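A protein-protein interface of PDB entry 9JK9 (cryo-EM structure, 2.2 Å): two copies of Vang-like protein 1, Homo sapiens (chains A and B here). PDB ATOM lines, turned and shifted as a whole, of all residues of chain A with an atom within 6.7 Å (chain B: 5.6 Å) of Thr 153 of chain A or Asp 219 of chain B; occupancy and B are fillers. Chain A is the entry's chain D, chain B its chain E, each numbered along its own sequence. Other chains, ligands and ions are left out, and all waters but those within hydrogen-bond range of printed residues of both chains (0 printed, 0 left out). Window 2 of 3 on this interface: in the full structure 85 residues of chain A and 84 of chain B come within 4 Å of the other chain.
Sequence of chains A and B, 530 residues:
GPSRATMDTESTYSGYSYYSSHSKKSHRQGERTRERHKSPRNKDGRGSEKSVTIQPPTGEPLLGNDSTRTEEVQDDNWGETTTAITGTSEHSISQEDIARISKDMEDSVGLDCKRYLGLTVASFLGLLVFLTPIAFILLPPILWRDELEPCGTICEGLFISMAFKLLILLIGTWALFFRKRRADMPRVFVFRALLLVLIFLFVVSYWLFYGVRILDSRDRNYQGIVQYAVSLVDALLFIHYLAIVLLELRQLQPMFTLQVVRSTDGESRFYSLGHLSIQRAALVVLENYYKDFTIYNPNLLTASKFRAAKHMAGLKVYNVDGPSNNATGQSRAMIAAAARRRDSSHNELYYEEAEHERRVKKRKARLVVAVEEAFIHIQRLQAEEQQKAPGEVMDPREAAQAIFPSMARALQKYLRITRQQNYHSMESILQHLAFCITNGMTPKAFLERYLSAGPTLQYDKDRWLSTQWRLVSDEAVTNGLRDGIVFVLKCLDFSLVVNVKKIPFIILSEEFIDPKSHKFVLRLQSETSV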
ATOM      1  N   PRO A 150     -18.976  40.691 -17.948  1.00  0.00           N
ATOM      2  CA  PRO A 150     -18.558  39.282 -17.905  1.00  0.00           C
ATOM      3  C   PRO A 150     -19.714  38.312 -18.114  1.00  0.00           C
ATOM      4  O   PRO A 150     -20.547  38.107 -17.225  1.00  0.00           O
ATOM      5  CB  PRO A 150     -17.941  39.142 -16.508  1.00  0.00           C
ATOM      6  CG  PRO A 150     -18.567  40.227 -15.700  1.00  0.00           C
ATOM      7  CD  PRO A 150     -18.795  41.365 -16.649  1.00  0.00           C
ATOM      8  N   CYS A 151     -19.767  37.711 -19.304  1.00  0.00           N
ATOM      9  CA  CYS A 151     -20.827  36.761 -19.624  1.00  0.00           C
ATOM     10  C   CYS A 151     -20.523  35.388 -19.040  1.00  0.00           C
ATOM     11  O   CYS A 151     -21.276  34.874 -18.205  1.00  0.00           O
ATOM     12  CB  CYS A 151     -21.009  36.674 -21.141  1.00  0.00           C
ATOM     13  SG  CYS A 151     -19.548  36.071 -22.030  1.00  0.00           S
ATOM     14  N   GLY A 152     -19.423  34.780 -19.469  1.00  0.00           N
ATOM     15  CA  GLY A 152     -19.003  33.510 -18.915  1.00  0.00           C
ATOM     16  C   GLY A 152     -19.679  32.306 -19.534  1.00  0.00           C
ATOM     17  O   GLY A 152     -19.324  31.877 -20.635  1.00  0.00           O
ATOM     18  N   THR A 153     -20.662  31.753 -18.824  1.00  0.00           N
ATOM     19  CA  THR A 153     -21.253  30.483 -19.232  1.00  0.00           C
ATOM     20  C   THR A 153     -22.264  30.661 -20.359  1.00  0.00           C
ATOM     21  O   THR A 153     -22.202  29.953 -21.374  1.00  0.00           O
ATOM     22  CB  THR A 153     -21.914  29.815 -18.028  1.00  0.00           C
ATOM     23  OG1 THR A 153     -20.925  29.545 -17.027  1.00  0.00           O
ATOM     24  CG2 THR A 153     -22.582  28.521 -18.436  1.00  0.00           C
ATOM     25  N   ILE A 154     -23.190  31.610 -20.204  1.00  0.00           N
ATOM     26  CA  ILE A 154     -24.380  31.652 -21.052  1.00  0.00           C
ATOM     27  C   ILE A 154     -24.019  32.108 -22.460  1.00  0.00           C
ATOM     28  O   ILE A 154     -24.562  31.599 -23.452  1.00  0.00           O
ATOM     29  CB  ILE A 154     -25.451  32.556 -20.411  1.00  0.00           C
ATOM     30  CG1 ILE A 154     -25.687  32.136 -18.959  1.00  0.00           C
ATOM     31  CG2 ILE A 154     -26.759  32.467 -21.175  1.00  0.00           C
ATOM     32  CD1 ILE A 154     -26.130  30.698 -18.797  1.00  0.00           C
ATOM     33  N   CYS A 155     -23.058  33.030 -22.569  1.00  0.00           N
ATOM     34  CA  CYS A 155     -22.593  33.482 -23.876  1.00  0.00           C
ATOM     35  C   CYS A 155     -21.920  32.354 -24.649  1.00  0.00           C
ATOM     36  O   CYS A 155     -22.165  32.195 -25.846  1.00  0.00           O
ATOM     37  CB  CYS A 155     -21.643  34.668 -23.716  1.00  0.00           C
ATOM     38  SG  CYS A 155     -20.114  34.297 -22.828  1.00  0.00           S
ATOM     39  N   GLU A 156     -21.126  31.521 -23.969  1.00  0.00           N
ATOM     40  CA  GLU A 156     -20.442  30.423 -24.652  1.00  0.00           C
ATOM     41  C   GLU A 156     -21.413  29.313 -25.040  1.00  0.00           C
ATOM     42  O   GLU A 156     -21.330  28.762 -26.150  1.00  0.00           O
ATOM     43  CB  GLU A 156     -19.317  29.882 -23.774  1.00  0.00           C
ATOM     44  CG  GLU A 156     -18.173  30.862 -23.588  1.00  0.00           C
ATOM     45  CD  GLU A 156     -17.102  30.329 -22.666  1.00  0.00           C
ATOM     46  OE1 GLU A 156     -17.314  29.249 -22.077  1.00  0.00           O
ATOM     47  OE2 GLU A 156     -16.051  30.990 -22.524  1.00  0.00           O
ATOM     48  N   GLY A 157     -22.360  28.994 -24.155  1.00  0.00           N
ATOM     49  CA  GLY A 157     -23.405  28.043 -24.495  1.00  0.00           C
ATOM     50  C   GLY A 157     -24.345  28.531 -25.573  1.00  0.00           C
ATOM     51  O   GLY A 157     -25.033  27.719 -26.200  1.00  0.00           O
ATOM     52  N   LEU A 158     -24.391  29.838 -25.799  1.00  0.00           N
ATOM     53  CA  LEU A 158     -25.127  30.379 -26.924  1.00  0.00           C
ATOM     54  C   LEU A 158     -24.280  30.426 -28.197  1.00  0.00           C
ATOM     55  O   LEU A 158     -24.829  30.291 -29.299  1.00  0.00           O
ATOM     56  CB  LEU A 158     -25.655  31.760 -26.534  1.00  0.00           C
ATOM     57  CG  LEU A 158     -26.768  32.421 -27.324  1.00  0.00           C
ATOM     58  CD1 LEU A 158     -27.993  31.528 -27.335  1.00  0.00           C
ATOM     59  CD2 LEU A 158     -27.104  33.730 -26.663  1.00  0.00           C
ATOM     60  N   TRP B 144     -27.829  21.657  -6.716  1.00  0.00           N
ATOM     61  CA  TRP B 144     -27.683  22.849  -5.872  1.00  0.00           C
ATOM     62  C   TRP B 144     -29.042  23.557  -5.810  1.00  0.00           C
ATOM     63  O   TRP B 144     -29.331  24.482  -6.562  1.00  0.00           O
ATOM     64  CB  TRP B 144     -26.514  23.769  -6.379  1.00  0.00           C
ATOM     65  CG  TRP B 144     -26.555  24.263  -7.824  1.00  0.00           C
ATOM     66  CD1 TRP B 144     -27.050  25.456  -8.277  1.00  0.00           C
ATOM     67  CD2 TRP B 144     -26.064  23.576  -8.983  1.00  0.00           C
ATOM     68  NE1 TRP B 144     -26.909  25.546  -9.638  1.00  0.00           N
ATOM     69  CE2 TRP B 144     -26.305  24.406 -10.097  1.00  0.00           C
ATOM     70  CE3 TRP B 144     -25.446  22.340  -9.188  1.00  0.00           C
ATOM     71  CZ2 TRP B 144     -25.953  24.039 -11.392  1.00  0.00           C
ATOM     72  CZ3 TRP B 144     -25.100  21.975 -10.476  1.00  0.00           C
ATOM     73  CH2 TRP B 144     -25.353  22.823 -11.561  1.00  0.00           C
ATOM     74  N   GLU B 147     -29.077  27.363  -4.360  1.00  0.00           N
ATOM     75  CA  GLU B 147     -28.204  28.313  -5.031  1.00  0.00           C
ATOM     76  C   GLU B 147     -28.879  28.977  -6.233  1.00  0.00           C
ATOM     77  O   GLU B 147     -28.330  29.941  -6.783  1.00  0.00           O
ATOM     78  CB  GLU B 147     -26.901  27.593  -5.439  1.00  0.00           C
ATOM     79  CG  GLU B 147     -25.701  28.484  -5.767  1.00  0.00           C
ATOM     80  CD  GLU B 147     -24.445  27.693  -6.081  1.00  0.00           C
ATOM     81  OE1 GLU B 147     -24.505  26.446  -6.072  1.00  0.00           O
ATOM     82  OE2 GLU B 147     -23.395  28.323  -6.335  1.00  0.00           O
ATOM     83  N   PHE B 209     -20.167  20.766 -22.586  1.00  0.00           N
ATOM     84  CA  PHE B 209     -20.263  22.113 -22.038  1.00  0.00           C
ATOM     85  C   PHE B 209     -21.101  22.145 -20.767  1.00  0.00           C
ATOM     86  O   PHE B 209     -20.859  22.982 -19.891  1.00  0.00           O
ATOM     87  CB  PHE B 209     -20.850  23.073 -23.069  1.00  0.00           C
ATOM     88  CG  PHE B 209     -20.802  24.504 -22.638  1.00  0.00           C
ATOM     89  CD1 PHE B 209     -19.622  25.220 -22.737  1.00  0.00           C
ATOM     90  CD2 PHE B 209     -21.918  25.125 -22.097  1.00  0.00           C
ATOM     91  CE1 PHE B 209     -19.561  26.532 -22.333  1.00  0.00           C
ATOM     92  CE2 PHE B 209     -21.855  26.431 -21.677  1.00  0.00           C
ATOM     93  CZ  PHE B 209     -20.677  27.135 -21.802  1.00  0.00           C
ATOM     94  N   ARG B 213     -18.659  23.437 -17.812  1.00  0.00           N
ATOM     95  CA  ARG B 213     -18.881  24.838 -17.489  1.00  0.00           C
ATOM     96  C   ARG B 213     -20.182  25.114 -16.751  1.00  0.00           C
ATOM     97  O   ARG B 213     -20.491  26.282 -16.502  1.00  0.00           O
ATOM     98  CB  ARG B 213     -18.830  25.685 -18.764  1.00  0.00           C
ATOM     99  CG  ARG B 213     -17.477  25.674 -19.447  1.00  0.00           C
ATOM    100  CD  ARG B 213     -16.424  26.312 -18.562  1.00  0.00           C
ATOM    101  NE  ARG B 213     -16.749  27.695 -18.229  1.00  0.00           N
ATOM    102  CZ  ARG B 213     -16.421  28.740 -18.979  1.00  0.00           C
ATOM    103  NH1 ARG B 213     -15.751  28.563 -20.108  1.00  0.00           N
ATOM    104  NH2 ARG B 213     -16.760  29.964 -18.597  1.00  0.00           N
ATOM    105  N   ILE B 214     -20.961  24.091 -16.400  1.00  0.00           N
ATOM    106  CA  ILE B 214     -22.179  24.316 -15.626  1.00  0.00           C
ATOM    107  C   ILE B 214     -22.172  23.465 -14.360  1.00  0.00           C
ATOM    108  O   ILE B 214     -22.366  23.984 -13.255  1.00  0.00           O
ATOM    109  CB  ILE B 214     -23.443  24.062 -16.473  1.00  0.00           C
ATOM    110  CG1 ILE B 214     -23.565  25.125 -17.568  1.00  0.00           C
ATOM    111  CG2 ILE B 214     -24.690  24.060 -15.606  1.00  0.00           C
ATOM    112  CD1 ILE B 214     -24.626  24.860 -18.601  1.00  0.00           C
ATOM    113  N   LEU B 215     -21.946  22.156 -14.503  1.00  0.00           N
ATOM    114  CA  LEU B 215     -21.974  21.280 -13.335  1.00  0.00           C
ATOM    115  C   LEU B 215     -20.727  21.432 -12.473  1.00  0.00           C
ATOM    116  O   LEU B 215     -20.827  21.461 -11.242  1.00  0.00           O
ATOM    117  CB  LEU B 215     -22.134  19.822 -13.760  1.00  0.00           C
ATOM    118  CG  LEU B 215     -23.476  19.433 -14.372  1.00  0.00           C
ATOM    119  CD1 LEU B 215     -23.461  17.972 -14.790  1.00  0.00           C
ATOM    120  CD2 LEU B 215     -24.611  19.715 -13.406  1.00  0.00           C
ATOM    121  N   SER B 217     -18.927  24.050 -12.208  1.00  0.00           N
ATOM    122  CA  SER B 217     -18.921  25.379 -11.618  1.00  0.00           C
ATOM    123  C   SER B 217     -20.097  25.623 -10.684  1.00  0.00           C
ATOM    124  O   SER B 217     -20.019  26.542  -9.859  1.00  0.00           O
ATOM    125  CB  SER B 217     -18.910  26.443 -12.718  1.00  0.00           C
ATOM    126  OG  SER B 217     -20.088  26.372 -13.496  1.00  0.00           O
ATOM    127  N   ARG B 218     -21.159  24.814 -10.794  1.00  0.00           N
ATOM    128  CA  ARG B 218     -22.390  24.903  -9.996  1.00  0.00           C
ATOM    129  C   ARG B 218     -23.007  26.301 -10.102  1.00  0.00           C
ATOM    130  O   ARG B 218     -23.054  27.076  -9.145  1.00  0.00           O
ATOM    131  CB  ARG B 218     -22.136  24.506  -8.535  1.00  0.00           C
ATOM    132  CG  ARG B 218     -21.775  23.042  -8.353  1.00  0.00           C
ATOM    133  CD  ARG B 218     -21.557  22.697  -6.890  1.00  0.00           C
ATOM    134  NE  ARG B 218     -21.113  21.315  -6.719  1.00  0.00           N
ATOM    135  CZ  ARG B 218     -21.933  20.281  -6.573  1.00  0.00           C
ATOM    136  NH1 ARG B 218     -23.245  20.468  -6.574  1.00  0.00           N
ATOM    137  NH2 ARG B 218     -21.443  19.056  -6.425  1.00  0.00           N
ATOM    138  N   ASP B 219     -23.466  26.597 -11.316  1.00  0.00           N
ATOM    139  CA  ASP B 219     -23.782  27.961 -11.710  1.00  0.00           C
ATOM    140  C   ASP B 219     -25.026  28.500 -11.013  1.00  0.00           C
ATOM    141  O   ASP B 219     -25.905  27.765 -10.559  1.00  0.00           O
ATOM    142  CB  ASP B 219     -23.995  28.059 -13.220  1.00  0.00           C
ATOM    143  CG  ASP B 219     -22.705  27.979 -13.997  1.00  0.00           C
ATOM    144  OD1 ASP B 219     -21.649  28.356 -13.446  1.00  0.00           O
ATOM    145  OD2 ASP B 219     -22.747  27.556 -15.168  1.00  0.00           O
ATOM    146  N   ARG B 220     -25.072  29.825 -10.947  1.00  0.00           N
ATOM    147  CA  ARG B 220     -26.257  30.609 -10.637  1.00  0.00           C
ATOM    148  C   ARG B 220     -27.035  30.833 -11.936  1.00  0.00           C
ATOM    149  O   ARG B 220     -26.905  30.031 -12.864  1.00  0.00           O
ATOM    150  CB  ARG B 220     -25.848  31.899  -9.926  1.00  0.00           C
ATOM    151  CG  ARG B 220     -25.236  31.635  -8.566  1.00  0.00           C
ATOM    152  CD  ARG B 220     -24.884  32.914  -7.836  1.00  0.00           C
ATOM    153  NE  ARG B 220     -24.218  32.626  -6.570  1.00  0.00           N
ATOM    154  CZ  ARG B 220     -24.853  32.401  -5.426  1.00  0.00           C
ATOM    155  NH1 ARG B 220     -26.179  32.429  -5.384  1.00  0.00           N
ATOM    156  NH2 ARG B 220     -24.165  32.146  -4.322  1.00  0.00           N
ATOM    157  N   ASN B 221     -27.913  31.845 -11.940  1.00  0.00           N
ATOM    158  CA  ASN B 221     -28.761  32.338 -13.050  1.00  0.00           C
ATOM    159  C   ASN B 221     -29.367  31.214 -13.899  1.00  0.00           C
ATOM    160  O   ASN B 221     -29.112  31.061 -15.093  1.00  0.00           O
ATOM    161  CB  ASN B 221     -28.070  33.448 -13.886  1.00  0.00           C
ATOM    162  CG  ASN B 221     -26.776  33.037 -14.623  1.00  0.00           C
ATOM    163  OD1 ASN B 221     -26.445  31.879 -14.814  1.00  0.00           O
ATOM    164  ND2 ASN B 221     -26.034  34.055 -15.046  1.00  0.00           N
ATOM    165  N   ILE B 225     -29.663  28.726 -17.764  1.00  0.00           N
ATOM    166  CA  ILE B 225     -29.613  27.281 -17.969  1.00  0.00           C
ATOM    167  C   ILE B 225     -30.836  26.817 -18.753  1.00  0.00           C
ATOM    168  O   ILE B 225     -30.738  25.958 -19.643  1.00  0.00           O
ATOM    169  CB  ILE B 225     -29.492  26.558 -16.614  1.00  0.00           C
ATOM    170  CG1 ILE B 225     -28.307  27.106 -15.819  1.00  0.00           C
ATOM    171  CG2 ILE B 225     -29.331  25.060 -16.807  1.00  0.00           C
ATOM    172  CD1 ILE B 225     -26.974  26.941 -16.505  1.00  0.00           C
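The side-chain carboxylate (OD2) of Asp 219 of chain B sits at hydrogen-bond distance from the side-chain hydroxyl (OG1) of Thr 153 of chain A. The guanidinium group (NH1) of Arg 213 of chain B is in salt-bridge range of the side-chain carboxylate (OE1) of Glu 156 of chain A, 2.6 Å away. The backbone carbonyl oxygen (O) of Arg 213 of chain B lies within hydrogen-bond range of the side-chain hydroxyl (OG1) of Thr 153 of chain A (3.3 Å).
The side-chain sulfur (SG) of Cys 151 of chain A is disulfide-bonded to the side-chain sulfur (SG) of Cys 155 of chain A, 2.0 Å away. The side-chain hydroxyl of Ser 217 of chain B is in hydrogen-bond range of the backbone carbonyl oxygen of Ile 214 of chain B. The backbone carbonyl oxygen (O) of Arg 213 of chain B is in hydrogen-bond range of the side-chain hydroxyl (OG) of Ser 217 of chain B, 3.0 Å away. O of Ile 214 of chain B is in hydrogen-bond range of N of Asp 219 of chain B (3.4 Å). The indole nitrogen (NE1) of Trp 144 of chain B sits at hydrogen-bond distance from the backbone carbonyl oxygen (O) of Asp 219 of chain B, 2.6 Å away. N of Gly 152 of chain A sits at hydrogen-bond distance from SG of Cys 155 of chain A.
Hydrophobic or aromatic side chains of chain B that line the printed part of chain A: Phe 209 and Ile 214. Along chain B the printed residues that touch a printed residue of chain A span positions 209 to 219. Among the printed residues, 8 pairs touch across the chains. Among the printed residues, Asp or Glu carboxylates within 4 Å of a Lys or Arg side-chain nitrogen of the other chain: Glu 156 of chain A with Arg 213 of chain B (2.6 Å).
Of chain B, only Phe 209 (3.2 Å), Arg 213 (3.3 Å), Ile 214 (3.6 Å) and Asp 219 (3.3 Å) come within 4 Å of Thr 153 of chain A. Printed residues of chain B within 4 Å of Glu 156 of chain A: Phe 209 (3.5 Å) and Arg 213 (2.6 Å). Of the printed residues of chain A, Ile 214 of chain B touches Thr 153. Leu 215 of chain B touches none of the printed residues of chain A. Asp 219 of chain B touches one residue of chain A. The nearest residue of chain A that does not touch Asp 219 of chain B is Ile 154 of chain A (5.9 Å).
No position is printed for both chains. Of the 8 pairs that touch across the chains among the printed residues, none has its exchanged pair printed and touching as well.
Among the printed residues, merely in contact across the chains: Gly 152 of chain A with Arg 213 of chain B, Thr 153 of chain A with Phe 209 of chain B, Thr 153 of chain A with Ile 214 of chain B, Glu 156 of chain A with Phe 209 of chain B and Gly 157 of chain A with Phe 209 of chain B.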
